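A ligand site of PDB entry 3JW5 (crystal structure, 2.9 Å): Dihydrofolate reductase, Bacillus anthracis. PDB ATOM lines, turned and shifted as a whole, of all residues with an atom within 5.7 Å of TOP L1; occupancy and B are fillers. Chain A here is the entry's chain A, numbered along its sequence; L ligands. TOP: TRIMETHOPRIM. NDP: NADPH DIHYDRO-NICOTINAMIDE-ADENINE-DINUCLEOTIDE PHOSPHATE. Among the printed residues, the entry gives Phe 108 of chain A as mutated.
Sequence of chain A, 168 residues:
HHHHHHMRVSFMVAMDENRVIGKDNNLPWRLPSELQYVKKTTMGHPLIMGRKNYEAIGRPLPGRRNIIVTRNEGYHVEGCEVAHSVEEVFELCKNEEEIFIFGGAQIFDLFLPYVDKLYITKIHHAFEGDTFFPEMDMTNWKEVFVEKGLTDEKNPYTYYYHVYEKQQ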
ATOM      1  N   MET A  12       9.833  30.522   8.590  1.00  0.00           N
ATOM      2  CA  MET A  12       9.223  30.252   7.301  1.00  0.00           C
ATOM      3  C   MET A  12       9.065  28.734   7.163  1.00  0.00           C
ATOM      4  O   MET A  12      10.058  28.012   7.198  1.00  0.00           O
ATOM      5  CB  MET A  12      10.127  30.793   6.194  1.00  0.00           C
ATOM      6  CG  MET A  12       9.603  30.574   4.787  1.00  0.00           C
ATOM      7  SD  MET A  12       7.939  31.212   4.546  1.00  0.00           S
ATOM      8  CE  MET A  12       8.173  32.980   4.673  1.00  0.00           C
ATOM      9  N   VAL A  13       7.834  28.271   7.010  1.00  0.00           N
ATOM     10  CA  VAL A  13       7.588  26.829   6.943  1.00  0.00           C
ATOM     11  C   VAL A  13       6.300  26.444   6.225  1.00  0.00           C
ATOM     12  O   VAL A  13       5.303  27.156   6.276  1.00  0.00           O
ATOM     13  CB  VAL A  13       7.689  26.154   8.359  1.00  0.00           C
ATOM     14  CG1 VAL A  13       6.502  26.551   9.270  1.00  0.00           C
ATOM     15  CG2 VAL A  13       7.812  24.638   8.251  1.00  0.00           C
ATOM     16  N   ALA A  14       6.335  25.299   5.542  1.00  0.00           N
ATOM     17  CA  ALA A  14       5.128  24.657   5.054  1.00  0.00           C
ATOM     18  C   ALA A  14       5.062  23.259   5.665  1.00  0.00           C
ATOM     19  O   ALA A  14       6.075  22.562   5.717  1.00  0.00           O
ATOM     20  CB  ALA A  14       5.131  24.592   3.546  1.00  0.00           C
ATOM     21  N   ASN A  25      14.921  13.591   2.688  1.00  0.00           N
ATOM     22  CA  ASN A  25      15.691  14.796   2.423  1.00  0.00           C
ATOM     23  C   ASN A  25      15.162  15.605   1.221  1.00  0.00           C
ATOM     24  O   ASN A  25      15.928  16.151   0.427  1.00  0.00           O
ATOM     25  CB  ASN A  25      17.187  14.482   2.305  1.00  0.00           C
ATOM     26  CG  ASN A  25      18.054  15.709   2.559  1.00  0.00           C
ATOM     27  OD1 ASN A  25      17.556  16.778   2.936  1.00  0.00           O
ATOM     28  ND2 ASN A  25      19.360  15.562   2.353  1.00  0.00           N
ATOM     29  N   ASN A  26      13.841  15.683   1.144  1.00  0.00           N
ATOM     30  CA  ASN A  26      13.177  16.322   0.026  1.00  0.00           C
ATOM     31  C   ASN A  26      11.771  16.729   0.450  1.00  0.00           C
ATOM     32  O   ASN A  26      11.195  16.107   1.348  1.00  0.00           O
ATOM     33  CB  ASN A  26      13.091  15.316  -1.118  1.00  0.00           C
ATOM     34  CG  ASN A  26      13.370  15.942  -2.465  1.00  0.00           C
ATOM     35  OD1 ASN A  26      13.848  17.066  -2.561  1.00  0.00           O
ATOM     36  ND2 ASN A  26      13.071  15.190  -3.525  1.00  0.00           N
ATOM     37  N   LEU A  27      11.215  17.758  -0.196  1.00  0.00           N
ATOM     38  CA  LEU A  27       9.821  18.153   0.015  1.00  0.00           C
ATOM     39  C   LEU A  27       8.853  17.085  -0.475  1.00  0.00           C
ATOM     40  O   LEU A  27       9.036  16.537  -1.566  1.00  0.00           O
ATOM     41  CB  LEU A  27       9.533  19.473  -0.695  1.00  0.00           C
ATOM     42  CG  LEU A  27       9.514  20.771   0.107  1.00  0.00           C
ATOM     43  CD1 LEU A  27      10.627  20.850   1.142  1.00  0.00           C
ATOM     44  CD2 LEU A  27       9.549  21.974  -0.827  1.00  0.00           C
ATOM     45  N   GLU A  34       3.243  28.305  -3.835  1.00  0.00           N
ATOM     46  CA  GLU A  34       3.635  28.450  -2.447  1.00  0.00           C
ATOM     47  C   GLU A  34       5.064  28.972  -2.380  1.00  0.00           C
ATOM     48  O   GLU A  34       5.374  29.814  -1.546  1.00  0.00           O
ATOM     49  CB  GLU A  34       3.528  27.129  -1.700  1.00  0.00           C
ATOM     50  CG  GLU A  34       3.360  27.265  -0.186  1.00  0.00           C
ATOM     51  CD  GLU A  34       4.680  27.377   0.589  1.00  0.00           C
ATOM     52  OE1 GLU A  34       5.746  27.054   0.023  1.00  0.00           O
ATOM     53  OE2 GLU A  34       4.636  27.791   1.768  1.00  0.00           O
ATOM     54  N   LEU A  35       5.902  28.475  -3.266  1.00  0.00           N
ATOM     55  CA  LEU A  35       7.282  28.951  -3.369  1.00  0.00           C
ATOM     56  C   LEU A  35       7.348  30.376  -3.878  1.00  0.00           C
ATOM     57  O   LEU A  35       8.252  31.117  -3.505  1.00  0.00           O
ATOM     58  CB  LEU A  35       8.114  28.038  -4.269  1.00  0.00           C
ATOM     59  CG  LEU A  35       8.773  26.826  -3.605  1.00  0.00           C
ATOM     60  CD1 LEU A  35       7.760  25.829  -2.998  1.00  0.00           C
ATOM     61  CD2 LEU A  35       9.656  26.121  -4.626  1.00  0.00           C
ATOM     62  N   VAL A  38       6.687  32.317  -0.845  1.00  0.00           N
ATOM     63  CA  VAL A  38       7.905  32.306  -0.028  1.00  0.00           C
ATOM     64  C   VAL A  38       8.913  33.304  -0.577  1.00  0.00           C
ATOM     65  O   VAL A  38       9.453  34.121   0.165  1.00  0.00           O
ATOM     66  CB  VAL A  38       8.539  30.891   0.076  1.00  0.00           C
ATOM     67  CG1 VAL A  38       9.915  30.970   0.690  1.00  0.00           C
ATOM     68  CG2 VAL A  38       7.659  29.962   0.885  1.00  0.00           C
ATOM     69  N   ASN A  53      19.241  21.141   4.706  1.00  0.00           N
ATOM     70  CA  ASN A  53      18.268  21.932   3.962  1.00  0.00           C
ATOM     71  C   ASN A  53      18.924  22.622   2.770  1.00  0.00           C
ATOM     72  O   ASN A  53      18.447  22.492   1.651  1.00  0.00           O
ATOM     73  CB  ASN A  53      17.565  22.959   4.863  1.00  0.00           C
ATOM     74  CG  ASN A  53      16.509  23.779   4.131  1.00  0.00           C
ATOM     75  OD1 ASN A  53      15.917  23.342   3.151  1.00  0.00           O
ATOM     76  ND2 ASN A  53      16.261  24.994   4.629  1.00  0.00           N
ATOM     77  N   ALA A  56      19.976  20.185  -0.141  1.00  0.00           N
ATOM     78  CA  ALA A  56      18.787  19.728  -0.867  1.00  0.00           C
ATOM     79  C   ALA A  56      18.348  20.783  -1.877  1.00  0.00           C
ATOM     80  O   ALA A  56      17.965  20.442  -2.986  1.00  0.00           O
ATOM     81  CB  ALA A  56      17.655  19.410   0.092  1.00  0.00           C
ATOM     82  N   ILE A  57      18.400  22.051  -1.469  1.00  0.00           N
ATOM     83  CA  ILE A  57      18.131  23.172  -2.379  1.00  0.00           C
ATOM     84  C   ILE A  57      19.233  23.310  -3.428  1.00  0.00           C
ATOM     85  O   ILE A  57      18.988  23.771  -4.533  1.00  0.00           O
ATOM     86  CB  ILE A  57      17.905  24.505  -1.610  1.00  0.00           C
ATOM     87  CG1 ILE A  57      16.705  24.379  -0.674  1.00  0.00           C
ATOM     88  CG2 ILE A  57      17.691  25.666  -2.565  1.00  0.00           C
ATOM     89  CD1 ILE A  57      16.688  25.405   0.469  1.00  0.00           C
ATOM     90  N   LEU A  61      20.013  31.088  -3.322  1.00  0.00           N
ATOM     91  CA  LEU A  61      18.775  31.708  -3.796  1.00  0.00           C
ATOM     92  C   LEU A  61      18.900  33.234  -3.902  1.00  0.00           C
ATOM     93  O   LEU A  61      19.272  33.891  -2.935  1.00  0.00           O
ATOM     94  CB  LEU A  61      17.591  31.307  -2.909  1.00  0.00           C
ATOM     95  CG  LEU A  61      17.223  29.816  -2.884  1.00  0.00           C
ATOM     96  CD1 LEU A  61      16.112  29.589  -1.859  1.00  0.00           C
ATOM     97  CD2 LEU A  61      16.833  29.266  -4.282  1.00  0.00           C
ATOM     98  N   ILE A 101      14.319  32.013   9.416  1.00  0.00           N
ATOM     99  CA  ILE A 101      14.718  30.661   9.720  1.00  0.00           C
ATOM    100  C   ILE A 101      13.950  29.787   8.752  1.00  0.00           C
ATOM    101  O   ILE A 101      12.723  29.782   8.731  1.00  0.00           O
ATOM    102  CB  ILE A 101      14.373  30.261  11.177  1.00  0.00           C
ATOM    103  CG1 ILE A 101      14.818  31.349  12.177  1.00  0.00           C
ATOM    104  CG2 ILE A 101      14.968  28.892  11.522  1.00  0.00           C
ATOM    105  CD1 ILE A 101      16.308  31.613  12.275  1.00  0.00           C
ATOM    106  N   PHE A 102      14.702  29.052   7.943  1.00  0.00           N
ATOM    107  CA  PHE A 102      14.158  28.461   6.757  1.00  0.00           C
ATOM    108  C   PHE A 102      14.163  26.937   6.801  1.00  0.00           C
ATOM    109  O   PHE A 102      13.587  26.290   5.924  1.00  0.00           O
ATOM    110  CB  PHE A 102      14.954  28.976   5.558  1.00  0.00           C
ATOM    111  CG  PHE A 102      14.238  28.844   4.271  1.00  0.00           C
ATOM    112  CD1 PHE A 102      13.162  29.679   3.959  1.00  0.00           C
ATOM    113  CD2 PHE A 102      14.632  27.889   3.337  1.00  0.00           C
ATOM    114  CE1 PHE A 102      12.492  29.562   2.754  1.00  0.00           C
ATOM    115  CE2 PHE A 102      13.970  27.766   2.133  1.00  0.00           C
ATOM    116  CZ  PHE A 102      12.893  28.603   1.843  1.00  0.00           C
ATOM    117  N   GLY A 103      14.788  26.365   7.833  1.00  0.00           N
ATOM    118  CA  GLY A 103      14.775  24.917   8.041  1.00  0.00           C
ATOM    119  C   GLY A 103      16.133  24.232   7.883  1.00  0.00           C
ATOM    120  O   GLY A 103      17.128  24.892   7.629  1.00  0.00           O
ATOM    121  N   PHE A 108      15.108  24.342  12.894  1.00  0.00           N
ATOM    122  CA  PHE A 108      13.910  24.849  13.576  1.00  0.00           C
ATOM    123  C   PHE A 108      14.047  24.680  15.103  1.00  0.00           C
ATOM    124  O   PHE A 108      13.804  25.630  15.846  1.00  0.00           O
ATOM    125  CB  PHE A 108      12.615  24.195  13.062  1.00  0.00           C
ATOM    126  CG  PHE A 108      12.188  24.659  11.680  1.00  0.00           C
ATOM    127  CD1 PHE A 108      11.839  23.739  10.689  1.00  0.00           C
ATOM    128  CD2 PHE A 108      12.107  26.019  11.357  1.00  0.00           C
ATOM    129  CE1 PHE A 108      11.447  24.151   9.410  1.00  0.00           C
ATOM    130  CE2 PHE A 108      11.715  26.444  10.073  1.00  0.00           C
ATOM    131  CZ  PHE A 108      11.387  25.506   9.107  1.00  0.00           C
ATOM    132  N   TYR A 119       5.437  32.451   9.879  1.00  0.00           N
ATOM    133  CA  TYR A 119       4.777  32.334   8.579  1.00  0.00           C
ATOM    134  C   TYR A 119       4.654  30.854   8.198  1.00  0.00           C
ATOM    135  O   TYR A 119       5.606  30.234   7.720  1.00  0.00           O
ATOM    136  CB  TYR A 119       5.546  33.088   7.496  1.00  0.00           C
ATOM    137  CG  TYR A 119       5.835  34.559   7.764  1.00  0.00           C
ATOM    138  CD1 TYR A 119       6.863  34.943   8.628  1.00  0.00           C
ATOM    139  CD2 TYR A 119       5.104  35.559   7.127  1.00  0.00           C
ATOM    140  CE1 TYR A 119       7.138  36.273   8.862  1.00  0.00           C
ATOM    141  CE2 TYR A 119       5.378  36.902   7.355  1.00  0.00           C
ATOM    142  CZ  TYR A 119       6.393  37.257   8.225  1.00  0.00           C
ATOM    143  OH  TYR A 119       6.672  38.590   8.445  1.00  0.00           O
ATOM    144  N   THR A 121       2.612  27.716   6.283  1.00  0.00           N
ATOM    145  CA  THR A 121       1.663  27.238   5.291  1.00  0.00           C
ATOM    146  C   THR A 121       1.144  25.867   5.705  1.00  0.00           C
ATOM    147  O   THR A 121       1.908  24.923   5.887  1.00  0.00           O
ATOM    148  CB  THR A 121       2.277  27.164   3.891  1.00  0.00           C
ATOM    149  OG1 THR A 121       2.821  28.437   3.548  1.00  0.00           O
ATOM    150  CG2 THR A 121       1.215  26.799   2.881  1.00  0.00           C
HETATM  151  C1  TOP L   1       9.241  25.768   1.713  1.00  0.00           C
HETATM  152  N2  TOP L   1       8.083  26.404   1.982  1.00  0.00           N
HETATM  153  C3  TOP L   1       7.894  27.145   3.112  1.00  0.00           C
HETATM  154  N4  TOP L   1       6.726  27.765   3.346  1.00  0.00           N
HETATM  155  N5  TOP L   1       8.881  27.278   4.011  1.00  0.00           N
HETATM  156  C6  TOP L   1      10.072  26.689   3.824  1.00  0.00           C
HETATM  157  N7  TOP L   1      11.009  26.862   4.776  1.00  0.00           N
HETATM  158  C8  TOP L   1      10.318  25.862   2.592  1.00  0.00           C
HETATM  159  C9  TOP L   1      11.670  25.181   2.388  1.00  0.00           C
HETATM  160  C10 TOP L   1      12.231  24.794   1.009  1.00  0.00           C
HETATM  161  C11 TOP L   1      12.208  25.688  -0.074  1.00  0.00           C
HETATM  162  C12 TOP L   1      12.734  25.348  -1.350  1.00  0.00           C
HETATM  163  O13 TOP L   1      12.700  26.217  -2.419  1.00  0.00           O
HETATM  164  C14 TOP L   1      12.275  27.577  -2.298  1.00  0.00           C
HETATM  165  C15 TOP L   1      13.344  24.005  -1.545  1.00  0.00           C
HETATM  166  O16 TOP L   1      13.904  23.607  -2.747  1.00  0.00           O
HETATM  167  C17 TOP L   1      13.150  23.427  -3.956  1.00  0.00           C
HETATM  168  C18 TOP L   1      13.370  23.081  -0.369  1.00  0.00           C
HETATM  169  O19 TOP L   1      13.932  21.814  -0.481  1.00  0.00           O
HETATM  170  C20 TOP L   1      13.580  20.871  -1.507  1.00  0.00           C
HETATM  171  C21 TOP L   1      12.818  23.520   0.858  1.00  0.00           C
HETATM  172  PA  NDP L   2      18.537  20.565   8.580  1.00  0.00           P
HETATM  173  O1A NDP L   2      17.997  21.055   9.871  1.00  0.00           O
HETATM  174  O2A NDP L   2      18.241  21.480   7.465  1.00  0.00           O
HETATM  175  O5B NDP L   2      20.106  20.361   8.686  1.00  0.00           O
HETATM  176  C5B NDP L   2      20.680  20.042   9.925  1.00  0.00           C
HETATM  177  C4B NDP L   2      22.166  20.301   9.776  1.00  0.00           C
HETATM  178  O4B NDP L   2      22.506  21.562  10.319  1.00  0.00           O
HETATM  179  C3B NDP L   2      23.000  19.260  10.493  1.00  0.00           C
HETATM  180  O3B NDP L   2      23.254  18.175   9.649  1.00  0.00           O
HETATM  181  C2B NDP L   2      24.241  20.069  10.804  1.00  0.00           C
HETATM  182  O2B NDP L   2      24.981  20.208   9.622  1.00  0.00           O
HETATM  183  C1B NDP L   2      23.697  21.452  11.075  1.00  0.00           C
HETATM  184  N9A NDP L   2      23.429  21.633  12.517  1.00  0.00           N
HETATM  185  C8A NDP L   2      22.422  21.067  13.267  1.00  0.00           C
HETATM  186  N7A NDP L   2      22.519  21.485  14.550  1.00  0.00           N
HETATM  187  C5A NDP L   2      23.575  22.314  14.622  1.00  0.00           C
HETATM  188  C6A NDP L   2      24.136  23.028  15.678  1.00  0.00           C
HETATM  189  N6A NDP L   2      23.579  22.930  16.878  1.00  0.00           N
HETATM  190  N1A NDP L   2      25.246  23.822  15.477  1.00  0.00           N
HETATM  191  C2A NDP L   2      25.814  23.908  14.211  1.00  0.00           C
HETATM  192  N3A NDP L   2      25.255  23.198  13.164  1.00  0.00           N
HETATM  193  C4A NDP L   2      24.160  22.420  13.364  1.00  0.00           C
HETATM  194  O3  NDP L   2      18.031  19.070   8.250  1.00  0.00           O
HETATM  195  PN  NDP L   2      16.792  18.188   8.780  1.00  0.00           P
HETATM  196  O1N NDP L   2      17.049  16.747   8.439  1.00  0.00           O
HETATM  197  O2N NDP L   2      16.533  18.599  10.183  1.00  0.00           O
HETATM  198  O5D NDP L   2      15.586  18.707   7.831  1.00  0.00           O
HETATM  199  C5D NDP L   2      15.633  18.541   6.436  1.00  0.00           C
HETATM  200  C4D NDP L   2      14.306  18.039   5.851  1.00  0.00           C
HETATM  201  O4D NDP L   2      13.286  19.010   6.007  1.00  0.00           O
HETATM  202  C3D NDP L   2      14.389  17.795   4.356  1.00  0.00           C
HETATM  203  O3D NDP L   2      13.513  16.728   4.009  1.00  0.00           O
HETATM  204  C2D NDP L   2      13.904  19.104   3.755  1.00  0.00           C
HETATM  205  O2D NDP L   2      13.449  18.928   2.434  1.00  0.00           O
HETATM  206  C1D NDP L   2      12.813  19.484   4.748  1.00  0.00           C
HETATM  207  N1N NDP L   2      12.449  20.909   4.843  1.00  0.00           N
HETATM  208  C2N NDP L   2      11.125  21.253   4.737  1.00  0.00           C
HETATM  209  C3N NDP L   2      10.701  22.582   4.838  1.00  0.00           C
HETATM  210  C7N NDP L   2       9.229  22.927   4.752  1.00  0.00           C
HETATM  211  O7N NDP L   2       8.801  24.231   5.047  1.00  0.00           O
HETATM  212  N7N NDP L   2       8.345  22.000   4.390  1.00  0.00           N
HETATM  213  C4N NDP L   2      11.650  23.566   5.064  1.00  0.00           C
HETATM  214  C5N NDP L   2      12.998  23.220   5.176  1.00  0.00           C
HETATM  215  C6N NDP L   2      13.392  21.887   5.074  1.00  0.00           C
HETATM  216  P2B NDP L   2      26.374  19.455   9.439  1.00  0.00           P
HETATM  217  O1X NDP L   2      27.331  20.034  10.451  1.00  0.00           O
HETATM  218  O2X NDP L   2      26.179  17.984   9.655  1.00  0.00           O
HETATM  219  O3X NDP L   2      26.889  19.662   8.054  1.00  0.00           O
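The side-chain carboxylate (OE2) of Glu 34 sits at hydrogen-bond distance from a nitrogen (N4) of TOP L1 (2.6 Å). O of Met 12 is in hydrogen-bond range of N7 of TOP L1, at 2.8 Å. The backbone carbonyl oxygen (O) of Phe 102 is in hydrogen-bond range of a nitrogen (N7) of TOP L1. N of Val 13 sits close to N5 of TOP L1, 3.3 Å away. O of Val 13 sits close to N4 of TOP L1, at 3.3 Å. An oxygen (O7N) of NDP L2 lies within hydrogen-bond range of the backbone NH of Ala 14 (2.7 Å). O of Ala 14 lies within hydrogen-bond range of N7N of NDP L2 (2.7 Å). The backbone NH (N) of Asn 53 lies within hydrogen-bond range of an oxygen (O2A) of NDP L2 (3.0 Å). An oxygen (O3D) of NDP L2 lies within hydrogen-bond range of the backbone NH (N) of Asn 26 (3.1 Å).
The backbone NH (N) of Ala 14 lies close to a nitrogen (N4) of TOP L1, 3.3 Å away. Residues that only touch TOP L1: Asn 26, Leu 27, Leu 35, Val 38, Asn 53, Ile 57 and Thr 121. Hydrophobic or aromatic side chains within 4 Å of TOP L1: Met 12, Ala 14, Leu 27, Leu 35, Val 38, Ile 57 and Phe 102. The nearest printed residue that does not touch TOP L1 is Leu 61 (4.4 Å).
O7N of NDP L2 lies close to N7 of TOP L1 (3.4 Å).
OE2 of Glu 34 lies within hydrogen-bond range of OG1 of Thr 121 (2.6 Å). The backbone carbonyl oxygen (O) of Ile 101 lies within hydrogen-bond range of the backbone NH (N) of Met 12 (3.0 Å). The side-chain amide nitrogen (ND2) of Asn 53 lies within hydrogen-bond range of the backbone carbonyl oxygen (O) of Phe 102 (3.2 Å). N of Thr 121 lies within hydrogen-bond range of O of Val 13, 2.7 Å away. The backbone NH of Val 13 sits at hydrogen-bond distance from the backbone carbonyl oxygen of Tyr 119, 3.1 Å away. ND2 of Asn 53 is in hydrogen-bond range of O of Gly 103, 3.1 Å away.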
